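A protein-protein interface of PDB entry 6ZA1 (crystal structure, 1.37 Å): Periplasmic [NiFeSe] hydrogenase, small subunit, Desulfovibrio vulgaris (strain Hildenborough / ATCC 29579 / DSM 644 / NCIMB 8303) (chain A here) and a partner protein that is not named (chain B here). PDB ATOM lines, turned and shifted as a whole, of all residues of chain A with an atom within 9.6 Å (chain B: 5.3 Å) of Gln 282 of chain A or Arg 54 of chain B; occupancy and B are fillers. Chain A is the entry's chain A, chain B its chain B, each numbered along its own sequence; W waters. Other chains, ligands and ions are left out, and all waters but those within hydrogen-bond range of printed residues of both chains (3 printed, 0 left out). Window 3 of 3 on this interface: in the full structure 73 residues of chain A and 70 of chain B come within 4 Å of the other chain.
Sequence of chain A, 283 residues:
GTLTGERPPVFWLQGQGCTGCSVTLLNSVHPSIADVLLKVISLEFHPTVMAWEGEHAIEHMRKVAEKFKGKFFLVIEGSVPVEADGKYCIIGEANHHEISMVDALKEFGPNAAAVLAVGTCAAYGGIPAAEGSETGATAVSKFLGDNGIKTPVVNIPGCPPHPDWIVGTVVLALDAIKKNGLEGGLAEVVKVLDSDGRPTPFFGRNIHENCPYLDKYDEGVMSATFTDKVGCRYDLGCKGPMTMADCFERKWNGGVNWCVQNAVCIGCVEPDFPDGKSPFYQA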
ATOM      1  N   ALA A 224      34.028 -25.402  10.394  1.00  0.00           N
ATOM      2  CA  ALA A 224      34.894 -25.084   9.269  1.00  0.00           C
ATOM      3  C   ALA A 224      34.623 -25.952   8.048  1.00  0.00           C
ATOM      4  O   ALA A 224      35.100 -25.624   6.956  1.00  0.00           O
ATOM      5  CB  ALA A 224      36.367 -25.233   9.667  1.00  0.00           C
ATOM      6  N   PHE A 226      31.291 -28.357   6.172  1.00  0.00           N
ATOM      7  CA  PHE A 226      29.843 -28.546   6.232  1.00  0.00           C
ATOM      8  C   PHE A 226      29.473 -29.749   7.098  1.00  0.00           C
ATOM      9  O   PHE A 226      28.422 -29.737   7.750  1.00  0.00           O
ATOM     10  CB  PHE A 226      29.255 -28.765   4.830  1.00  0.00           C
ATOM     11  CG  PHE A 226      29.249 -27.539   3.960  1.00  0.00           C
ATOM     12  CD1 PHE A 226      28.344 -26.515   4.183  1.00  0.00           C
ATOM     13  CD2 PHE A 226      30.136 -27.425   2.904  1.00  0.00           C
ATOM     14  CE1 PHE A 226      28.342 -25.391   3.377  1.00  0.00           C
ATOM     15  CE2 PHE A 226      30.133 -26.305   2.097  1.00  0.00           C
ATOM     16  CZ  PHE A 226      29.236 -25.289   2.333  1.00  0.00           C
ATOM     17  N   ARG A 233      26.838 -22.577  11.920  1.00  0.00           N
ATOM     18  CA  ARG A 233      27.047 -22.577  10.478  1.00  0.00           C
ATOM     19  C   ARG A 233      27.307 -21.180   9.913  1.00  0.00           C
ATOM     20  O   ARG A 233      27.388 -21.021   8.690  1.00  0.00           O
ATOM     21  CB  ARG A 233      25.829 -23.196   9.778  1.00  0.00           C
ATOM     22  CG  ARG A 233      25.675 -24.718   9.873  1.00  0.00           C
ATOM     23  CD  ARG A 233      25.341 -25.246  11.271  1.00  0.00           C
ATOM     24  NE  ARG A 233      24.688 -26.551  11.158  1.00  0.00           N
ATOM     25  CZ  ARG A 233      24.777 -27.549  12.032  1.00  0.00           C
ATOM     26  NH1 ARG A 233      25.511 -27.437  13.134  1.00  0.00           N
ATOM     27  NH2 ARG A 233      24.126 -28.677  11.791  1.00  0.00           N
ATOM     28  N   TYR A 234      27.463 -20.171  10.769  1.00  0.00           N
ATOM     29  CA  TYR A 234      27.587 -18.798  10.290  1.00  0.00           C
ATOM     30  C   TYR A 234      28.765 -18.623   9.341  1.00  0.00           C
ATOM     31  O   TYR A 234      28.636 -17.966   8.302  1.00  0.00           O
ATOM     32  CB  TYR A 234      27.743 -17.867  11.484  1.00  0.00           C
ATOM     33  CG  TYR A 234      27.838 -16.410  11.131  1.00  0.00           C
ATOM     34  CD1 TYR A 234      26.698 -15.670  10.872  1.00  0.00           C
ATOM     35  CD2 TYR A 234      29.064 -15.772  11.084  1.00  0.00           C
ATOM     36  CE1 TYR A 234      26.777 -14.333  10.562  1.00  0.00           C
ATOM     37  CE2 TYR A 234      29.157 -14.437  10.777  1.00  0.00           C
ATOM     38  CZ  TYR A 234      28.011 -13.719  10.517  1.00  0.00           C
ATOM     39  OH  TYR A 234      28.110 -12.385  10.210  1.00  0.00           O
ATOM     40  N   ASP A 235      29.930 -19.172   9.688  1.00  0.00           N
ATOM     41  CA  ASP A 235      31.103 -18.963   8.845  1.00  0.00           C
ATOM     42  C   ASP A 235      30.971 -19.672   7.506  1.00  0.00           C
ATOM     43  O   ASP A 235      31.643 -19.288   6.539  1.00  0.00           O
ATOM     44  CB  ASP A 235      32.367 -19.430   9.562  1.00  0.00           C
ATOM     45  CG  ASP A 235      32.867 -18.421  10.582  1.00  0.00           C
ATOM     46  OD1 ASP A 235      32.309 -17.305  10.657  1.00  0.00           O
ATOM     47  OD2 ASP A 235      33.827 -18.747  11.309  1.00  0.00           O
ATOM     48  N   LEU A 236      30.132 -20.697   7.433  1.00  0.00           N
ATOM     49  CA  LEU A 236      29.860 -21.405   6.190  1.00  0.00           C
ATOM     50  C   LEU A 236      28.832 -20.692   5.329  1.00  0.00           C
ATOM     51  O   LEU A 236      28.554 -21.150   4.213  1.00  0.00           O
ATOM     52  CB  LEU A 236      29.359 -22.809   6.516  1.00  0.00           C
ATOM     53  CG  LEU A 236      30.370 -23.765   7.141  1.00  0.00           C
ATOM     54  CD1 LEU A 236      29.617 -24.951   7.711  1.00  0.00           C
ATOM     55  CD2 LEU A 236      31.385 -24.204   6.117  1.00  0.00           C
ATOM     56  N   GLY A 237      28.251 -19.604   5.830  1.00  0.00           N
ATOM     57  CA  GLY A 237      27.352 -18.765   5.054  1.00  0.00           C
ATOM     58  C   GLY A 237      25.927 -18.696   5.555  1.00  0.00           C
ATOM     59  O   GLY A 237      25.086 -18.087   4.878  1.00  0.00           O
ATOM     60  N   CYS A 238      25.595 -19.262   6.711  1.00  0.00           N
ATOM     61  CA  CYS A 238      24.211 -19.285   7.165  1.00  0.00           C
ATOM     62  C   CYS A 238      23.620 -17.881   7.248  1.00  0.00           C
ATOM     63  O   CYS A 238      24.207 -16.980   7.855  1.00  0.00           O
ATOM     64  CB  CYS A 238      24.135 -19.952   8.536  1.00  0.00           C
ATOM     65  SG  CYS A 238      22.452 -20.197   9.098  1.00  0.00           S
ATOM     66  N   LYS A 239      22.447 -17.708   6.637  1.00  0.00           N
ATOM     67  CA  LYS A 239      21.723 -16.443   6.630  1.00  0.00           C
ATOM     68  C   LYS A 239      20.570 -16.427   7.624  1.00  0.00           C
ATOM     69  O   LYS A 239      19.716 -15.532   7.565  1.00  0.00           O
ATOM     70  CB  LYS A 239      21.226 -16.135   5.216  1.00  0.00           C
ATOM     71  CG  LYS A 239      22.333 -16.086   4.160  1.00  0.00           C
ATOM     72  CD  LYS A 239      23.451 -15.122   4.560  1.00  0.00           C
ATOM     73  CE  LYS A 239      24.407 -14.833   3.409  1.00  0.00           C
ATOM     74  NZ  LYS A 239      25.133 -16.053   2.958  1.00  0.00           N
ATOM     75  N   VAL A 264      23.274 -24.891   5.231  1.00  0.00           N
ATOM     76  CA  VAL A 264      23.069 -23.524   5.692  1.00  0.00           C
ATOM     77  C   VAL A 264      21.686 -23.053   5.252  1.00  0.00           C
ATOM     78  O   VAL A 264      21.117 -23.550   4.281  1.00  0.00           O
ATOM     79  CB  VAL A 264      24.141 -22.552   5.136  1.00  0.00           C
ATOM     80  CG1 VAL A 264      25.544 -22.971   5.565  1.00  0.00           C
ATOM     81  CG2 VAL A 264      24.051 -22.467   3.605  1.00  0.00           C
ATOM     82  N   CYS A 265      21.143 -22.074   5.980  1.00  0.00           N
ATOM     83  CA  CYS A 265      19.989 -21.324   5.500  1.00  0.00           C
ATOM     84  C   CYS A 265      20.463 -20.286   4.488  1.00  0.00           C
ATOM     85  O   CYS A 265      21.483 -19.622   4.704  1.00  0.00           O
ATOM     86  CB  CYS A 265      19.297 -20.624   6.673  1.00  0.00           C
ATOM     87  SG  CYS A 265      17.926 -19.517   6.270  1.00  0.00           S
ATOM     88  N   ILE A 266      19.738 -20.161   3.377  1.00  0.00           N
ATOM     89  CA  ILE A 266      20.056 -19.192   2.330  1.00  0.00           C
ATOM     90  C   ILE A 266      19.066 -18.029   2.307  1.00  0.00           C
ATOM     91  O   ILE A 266      19.100 -17.205   1.384  1.00  0.00           O
ATOM     92  CB  ILE A 266      20.215 -19.848   0.945  1.00  0.00           C
ATOM     93  CG1 ILE A 266      18.900 -20.457   0.449  1.00  0.00           C
ATOM     94  CG2 ILE A 266      21.320 -20.923   0.984  1.00  0.00           C
ATOM     95  CD1 ILE A 266      18.999 -21.017  -0.965  1.00  0.00           C
ATOM     96  N   GLY A 276      20.490 -10.204  -2.103  1.00  0.00           N
ATOM     97  CA  GLY A 276      20.822  -9.745  -0.767  1.00  0.00           C
ATOM     98  C   GLY A 276      21.236 -10.827   0.205  1.00  0.00           C
ATOM     99  O   GLY A 276      21.617 -10.535   1.343  1.00  0.00           O
ATOM    100  N   LYS A 277      21.160 -12.083  -0.227  1.00  0.00           N
ATOM    101  CA  LYS A 277      21.560 -13.235   0.567  1.00  0.00           C
ATOM    102  C   LYS A 277      22.776 -13.945  -0.027  1.00  0.00           C
ATOM    103  O   LYS A 277      23.127 -15.041   0.422  1.00  0.00           O
ATOM    104  CB  LYS A 277      20.389 -14.219   0.681  1.00  0.00           C
ATOM    105  CG  LYS A 277      19.168 -13.692   1.439  1.00  0.00           C
ATOM    106  CD  LYS A 277      19.459 -13.514   2.925  1.00  0.00           C
ATOM    107  CE  LYS A 277      18.243 -12.994   3.674  1.00  0.00           C
ATOM    108  NZ  LYS A 277      18.119 -11.517   3.549  1.00  0.00           N
ATOM    109  N   SER A 278      23.414 -13.347  -1.033  1.00  0.00           N
ATOM    110  CA  SER A 278      24.532 -13.917  -1.766  1.00  0.00           C
ATOM    111  C   SER A 278      25.800 -13.131  -1.477  1.00  0.00           C
ATOM    112  O   SER A 278      25.731 -11.929  -1.213  1.00  0.00           O
ATOM    113  CB  SER A 278      24.254 -13.801  -3.268  1.00  0.00           C
ATOM    114  OG  SER A 278      23.131 -14.570  -3.653  1.00  0.00           O
ATOM    115  N   PRO A 279      26.986 -13.766  -1.524  1.00  0.00           N
ATOM    116  CA  PRO A 279      27.248 -15.194  -1.765  1.00  0.00           C
ATOM    117  C   PRO A 279      26.659 -16.075  -0.677  1.00  0.00           C
ATOM    118  O   PRO A 279      26.633 -15.697   0.495  1.00  0.00           O
ATOM    119  CB  PRO A 279      28.782 -15.286  -1.742  1.00  0.00           C
ATOM    120  CG  PRO A 279      29.250 -13.904  -2.077  1.00  0.00           C
ATOM    121  CD  PRO A 279      28.237 -12.994  -1.424  1.00  0.00           C
ATOM    122  N   PHE A 280      26.180 -17.255  -1.072  1.00  0.00           N
ATOM    123  CA  PHE A 280      25.514 -18.121  -0.115  1.00  0.00           C
ATOM    124  C   PHE A 280      26.493 -18.749   0.870  1.00  0.00           C
ATOM    125  O   PHE A 280      26.109 -19.058   2.003  1.00  0.00           O
ATOM    126  CB  PHE A 280      24.754 -19.231  -0.842  1.00  0.00           C
ATOM    127  CG  PHE A 280      23.587 -18.747  -1.643  1.00  0.00           C
ATOM    128  CD1 PHE A 280      22.636 -17.917  -1.076  1.00  0.00           C
ATOM    129  CD2 PHE A 280      23.441 -19.112  -2.967  1.00  0.00           C
ATOM    130  CE1 PHE A 280      21.566 -17.467  -1.811  1.00  0.00           C
ATOM    131  CE2 PHE A 280      22.378 -18.666  -3.707  1.00  0.00           C
ATOM    132  CZ  PHE A 280      21.435 -17.843  -3.131  1.00  0.00           C
ATOM    133  N   TYR A 281      27.747 -18.947   0.473  1.00  0.00           N
ATOM    134  CA  TYR A 281      28.664 -19.778   1.244  1.00  0.00           C
ATOM    135  C   TYR A 281      29.805 -18.997   1.879  1.00  0.00           C
ATOM    136  O   TYR A 281      30.852 -19.571   2.188  1.00  0.00           O
ATOM    137  CB  TYR A 281      29.169 -20.924   0.379  1.00  0.00           C
ATOM    138  CG  TYR A 281      28.032 -21.830  -0.006  1.00  0.00           C
ATOM    139  CD1 TYR A 281      27.362 -22.575   0.957  1.00  0.00           C
ATOM    140  CD2 TYR A 281      27.605 -21.920  -1.320  1.00  0.00           C
ATOM    141  CE1 TYR A 281      26.314 -23.402   0.616  1.00  0.00           C
ATOM    142  CE2 TYR A 281      26.559 -22.744  -1.672  1.00  0.00           C
ATOM    143  CZ  TYR A 281      25.917 -23.483  -0.702  1.00  0.00           C
ATOM    144  OH  TYR A 281      24.873 -24.305  -1.062  1.00  0.00           O
ATOM    145  N   GLN A 282      29.611 -17.709   2.102  1.00  0.00           N
ATOM    146  CA  GLN A 282      30.465 -16.952   3.002  1.00  0.00           C
ATOM    147  C   GLN A 282      29.580 -15.975   3.758  1.00  0.00           C
ATOM    148  O   GLN A 282      28.484 -15.627   3.310  1.00  0.00           O
ATOM    149  CB  GLN A 282      31.632 -16.285   2.278  1.00  0.00           C
ATOM    150  CG  GLN A 282      31.292 -15.579   1.003  1.00  0.00           C
ATOM    151  CD  GLN A 282      32.538 -15.116   0.280  1.00  0.00           C
ATOM    152  OE1 GLN A 282      33.220 -15.905  -0.377  1.00  0.00           O
ATOM    153  NE2 GLN A 282      32.850 -13.832   0.407  1.00  0.00           N
ATOM    154  N   ALA A 283      30.037 -15.590   4.943  1.00  0.00           N
ATOM    155  CA  ALA A 283      29.266 -14.682   5.781  1.00  0.00           C
ATOM    156  C   ALA A 283      29.350 -13.300   5.144  1.00  0.00           C
ATOM    157  O   ALA A 283      28.410 -12.507   5.189  1.00  0.00           O
ATOM    158  CB  ALA A 283      29.803 -14.662   7.188  1.00  0.00           C
ATOM    159  OXT ALA A 283      30.377 -12.958   4.554  1.00  0.00           O
ATOM    160  N   ASP B  52      29.721 -15.523  -7.220  1.00  0.00           N
ATOM    161  CA  ASP B  52      30.546 -16.570  -6.635  1.00  0.00           C
ATOM    162  C   ASP B  52      30.154 -17.895  -7.279  1.00  0.00           C
ATOM    163  O   ASP B  52      28.968 -18.253  -7.261  1.00  0.00           O
ATOM    164  CB  ASP B  52      30.240 -16.600  -5.135  1.00  0.00           C
ATOM    165  CG  ASP B  52      31.100 -17.604  -4.345  1.00  0.00           C
ATOM    166  OD1 ASP B  52      31.480 -18.670  -4.878  1.00  0.00           O
ATOM    167  OD2 ASP B  52      31.367 -17.331  -3.153  1.00  0.00           O
ATOM    168  N   PRO B  53      31.097 -18.631  -7.883  1.00  0.00           N
ATOM    169  CA  PRO B  53      30.700 -19.872  -8.574  1.00  0.00           C
ATOM    170  C   PRO B  53      29.952 -20.853  -7.691  1.00  0.00           C
ATOM    171  O   PRO B  53      29.085 -21.587  -8.187  1.00  0.00           O
ATOM    172  CB  PRO B  53      32.034 -20.447  -9.073  1.00  0.00           C
ATOM    173  CG  PRO B  53      32.936 -19.251  -9.187  1.00  0.00           C
ATOM    174  CD  PRO B  53      32.534 -18.330  -8.055  1.00  0.00           C
ATOM    175  N   ARG B  54      30.247 -20.879  -6.389  1.00  0.00           N
ATOM    176  CA  ARG B  54      29.577 -21.826  -5.506  1.00  0.00           C
ATOM    177  C   ARG B  54      28.084 -21.534  -5.407  1.00  0.00           C
ATOM    178  O   ARG B  54      27.295 -22.433  -5.086  1.00  0.00           O
ATOM    179  CB  ARG B  54      30.201 -21.780  -4.115  1.00  0.00           C
ATOM    180  CG  ARG B  54      31.646 -22.202  -4.078  1.00  0.00           C
ATOM    181  CD  ARG B  54      32.256 -21.899  -2.730  1.00  0.00           C
ATOM    182  NE  ARG B  54      32.340 -20.461  -2.497  1.00  0.00           N
ATOM    183  CZ  ARG B  54      32.851 -19.912  -1.401  1.00  0.00           C
ATOM    184  NH1 ARG B  54      33.327 -20.685  -0.435  1.00  0.00           N
ATOM    185  NH2 ARG B  54      32.887 -18.594  -1.271  1.00  0.00           N
ATOM    186  N   ASP B  55      27.680 -20.285  -5.631  1.00  0.00           N
ATOM    187  CA  ASP B  55      26.252 -19.983  -5.607  1.00  0.00           C
ATOM    188  C   ASP B  55      25.501 -20.761  -6.678  1.00  0.00           C
ATOM    189  O   ASP B  55      24.287 -20.974  -6.556  1.00  0.00           O
ATOM    190  CB  ASP B  55      25.994 -18.501  -5.857  1.00  0.00           C
ATOM    191  CG  ASP B  55      26.384 -17.618  -4.694  1.00  0.00           C
ATOM    192  OD1 ASP B  55      26.797 -18.132  -3.631  1.00  0.00           O
ATOM    193  OD2 ASP B  55      26.268 -16.388  -4.860  1.00  0.00           O
ATOM    194  N   ALA B  56      26.186 -21.172  -7.747  1.00  0.00           N
ATOM    195  CA  ALA B  56      25.481 -21.793  -8.870  1.00  0.00           C
ATOM    196  C   ALA B  56      24.700 -23.022  -8.431  1.00  0.00           C
ATOM    197  O   ALA B  56      23.602 -23.279  -8.936  1.00  0.00           O
ATOM    198  CB  ALA B  56      26.456 -22.162  -9.988  1.00  0.00           C
ATOM    199  N   SER B  57      25.260 -23.822  -7.512  1.00  0.00           N
ATOM    200  CA  SER B  57      24.627 -25.089  -7.148  1.00  0.00           C
ATOM    201  C   SER B  57      23.331 -24.890  -6.367  1.00  0.00           C
ATOM    202  O   SER B  57      22.578 -25.858  -6.200  1.00  0.00           O
ATOM    203  CB  SER B  57      25.610 -26.005  -6.414  1.00  0.00           C
ATOM    204  OG  SER B  57      26.211 -25.379  -5.301  1.00  0.00           O
ATOM    205  N   GLN B  58      23.048 -23.672  -5.915  1.00  0.00           N
ATOM    206  CA  GLN B  58      21.722 -23.312  -5.428  1.00  0.00           C
ATOM    207  C   GLN B  58      20.889 -22.634  -6.511  1.00  0.00           C
ATOM    208  O   GLN B  58      19.739 -23.025  -6.749  1.00  0.00           O
ATOM    209  CB  GLN B  58      21.841 -22.414  -4.194  1.00  0.00           C
ATOM    210  CG  GLN B  58      22.255 -23.165  -2.943  1.00  0.00           C
ATOM    211  CD  GLN B  58      21.281 -24.270  -2.595  1.00  0.00           C
ATOM    212  OE1 GLN B  58      20.089 -24.022  -2.409  1.00  0.00           O
ATOM    213  NE2 GLN B  58      21.773 -25.500  -2.541  1.00  0.00           N
ATOM    214  N   LEU B  79      31.445 -27.703 -11.051  1.00  0.00           N
ATOM    215  CA  LEU B  79      32.285 -27.020 -10.074  1.00  0.00           C
ATOM    216  C   LEU B  79      33.389 -27.932  -9.555  1.00  0.00           C
ATOM    217  O   LEU B  79      34.523 -27.476  -9.355  1.00  0.00           O
ATOM    218  CB  LEU B  79      31.427 -26.516  -8.914  1.00  0.00           C
ATOM    219  CG  LEU B  79      30.387 -25.464  -9.280  1.00  0.00           C
ATOM    220  CD1 LEU B  79      29.421 -25.233  -8.125  1.00  0.00           C
ATOM    221  CD2 LEU B  79      31.056 -24.158  -9.669  1.00  0.00           C
ATOM    222  N   PHE B  83      37.066 -26.598  -9.931  1.00  0.00           N
ATOM    223  CA  PHE B  83      37.828 -26.331  -8.720  1.00  0.00           C
ATOM    224  C   PHE B  83      38.913 -27.374  -8.466  1.00  0.00           C
ATOM    225  O   PHE B  83      39.808 -27.137  -7.648  1.00  0.00           O
ATOM    226  CB  PHE B  83      36.937 -26.378  -7.472  1.00  0.00           C
ATOM    227  CG  PHE B  83      36.057 -25.170  -7.256  1.00  0.00           C
ATOM    228  CD1 PHE B  83      35.401 -24.550  -8.302  1.00  0.00           C
ATOM    229  CD2 PHE B  83      35.834 -24.701  -5.966  1.00  0.00           C
ATOM    230  CE1 PHE B  83      34.564 -23.461  -8.069  1.00  0.00           C
ATOM    231  CE2 PHE B  83      35.001 -23.615  -5.729  1.00  0.00           C
ATOM    232  CZ  PHE B  83      34.365 -22.998  -6.783  1.00  0.00           C
ATOM    233  N   VAL B 180      29.944 -28.188  -4.228  1.00  0.00           N
ATOM    234  CA  VAL B 180      31.267 -28.535  -4.737  1.00  0.00           C
ATOM    235  C   VAL B 180      32.014 -29.256  -3.626  1.00  0.00           C
ATOM    236  O   VAL B 180      31.978 -28.836  -2.467  1.00  0.00           O
ATOM    237  CB  VAL B 180      32.011 -27.283  -5.237  1.00  0.00           C
ATOM    238  CG1 VAL B 180      32.329 -26.314  -4.107  1.00  0.00           C
ATOM    239  CG2 VAL B 180      33.290 -27.698  -5.958  1.00  0.00           C
ATOM    240  N   VAL B 397      38.117 -21.416  -3.851  1.00  0.00           N
ATOM    241  CA  VAL B 397      37.574 -20.962  -5.136  1.00  0.00           C
ATOM    242  C   VAL B 397      38.727 -20.536  -6.039  1.00  0.00           C
ATOM    243  O   VAL B 397      39.543 -19.688  -5.635  1.00  0.00           O
ATOM    244  CB  VAL B 397      36.603 -19.801  -4.919  1.00  0.00           C
ATOM    245  CG1 VAL B 397      36.102 -19.289  -6.262  1.00  0.00           C
ATOM    246  CG2 VAL B 397      35.448 -20.214  -4.030  1.00  0.00           C
HETATM  247  O   HOH W   1      24.722 -26.025  -3.118  1.00  0.00           O
HETATM  248  O   HOH W   2      29.006 -18.780  -2.223  1.00  0.00           O
HETATM  249  O   HOH W   3      23.797 -15.858  -5.918  1.00  0.00           O
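The guanidinium group (NH2) of Arg 54 of chain B sits at hydrogen-bond distance from the side-chain amide oxygen (OE1) of Gln 282 of chain A (2.9 Å).
N of Phe 280 of chain A sits at hydrogen-bond distance from OD1 of Asp 55 of chain B.
The guanidinium group (NH2) of Arg 54 of chain B is in salt-bridge range of the side-chain carboxylate (OD2) of Asp 52 of chain B (2.7 Å).
The backbone carbonyl oxygen (O) of Gln 282 of chain A is in hydrogen-bond range of the side-chain amino group (NZ) of Lys 239 of chain A, 3.4 Å away.
The backbone carbonyl oxygen (O) of Phe 280 of chain A sits at hydrogen-bond distance from the side-chain amino group (NZ) of Lys 239 of chain A (3.3 Å).
The backbone carbonyl oxygen of Pro 279 of chain A lies within hydrogen-bond range of the side-chain amino group of Lys 239 of chain A, at 2.9 Å.
The backbone carbonyl oxygen (O) of Arg 54 of chain B lies within hydrogen-bond range of the side-chain hydroxyl (OG) of Ser 57 of chain B (3.1 Å).
Gln 58 of chain B touches Ile 266 of chain A (OE1 to CD1, 3.5 Å).
Ser 278 of chain A touches Asp 55 of chain B.
Asp 52 of chain B touches Pro 279 of chain A (OD2 to CB, 3.6 Å).
Pro 279 of chain A touches Asp 55 of chain B.
CE2 of Phe 280 of chain A touches CB of Gln 58 of chain B (3.8 Å).
CE2 of Tyr 281 of chain A touches O of Arg 54 of chain B, 3.5 Å away.
CG of Gln 58 of chain B touches OH of Tyr 281 of chain A, at 3.4 Å.
OE1 of Gln 282 of chain A touches OD2 of Asp 52 of chain B, at 3.6 Å.
Of the printed residues of chain B, Gln 282 of chain A touches Asp 52 and Arg 54.
Arg 54 of chain B touches just these residues of chain A: Tyr 281 and Gln 282.
Asp 52 of chain B touches just these residues of chain A: Pro 279 and Gln 282.
No residue of chain A comes within 4 Å of Pro 53 of chain B.
Ala 56 of chain B touches none of the printed residues of chain A.
Of the printed residues of chain B, Tyr 281 of chain A touches Arg 54 (3.5 Å) and Gln 58 (3.4 Å).
Of the printed residues of chain B, Phe 280 of chain A touches Asp 55 (2.8 Å) and Gln 58 (3.8 Å).
Of the printed residues of chain B, Pro 279 of chain A touches Asp 52 and Asp 55.
Of the printed residues of chain B, Ile 266 of chain A touches Gln 58.
Of the printed residues of chain B, Ser 278 of chain A touches Asp 55.
Ala 283 of chain A touches none of the printed residues of chain B.
The nearest printed residue of chain B that does not touch Gln 282 of chain A is Val 397 of chain B (6.1 Å).
The nearest residue of chain A that does not touch Arg 54 of chain B is Pro 279 of chain A (5.3 Å).
Among the printed residues, 10 pairs touch across the chains.
Among the printed residues, no Asp or Glu carboxylate lies within 4 Å of a Lys or Arg side-chain nitrogen of the other chain.
Water W1 lies within hydrogen-bond range of the side-chain hydroxyl of Tyr 281 of chain A, the side-chain hydroxyl of Ser 57 of chain B and the side-chain amide nitrogen of Gln 58 of chain B.
Water W3 lies within hydrogen-bond range of OG of Ser 278 of chain A (2.7 Å) and OD2 of Asp 55 of chain B (2.7 Å).
Water W2 lies within hydrogen-bond range of OD1 of Asp 55 of chain B (2.7 Å), OD2 of Asp 52 of chain B (2.9 Å), N of Tyr 281 of chain A (3.0 Å) and N of Phe 280 of chain A (3.4 Å).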
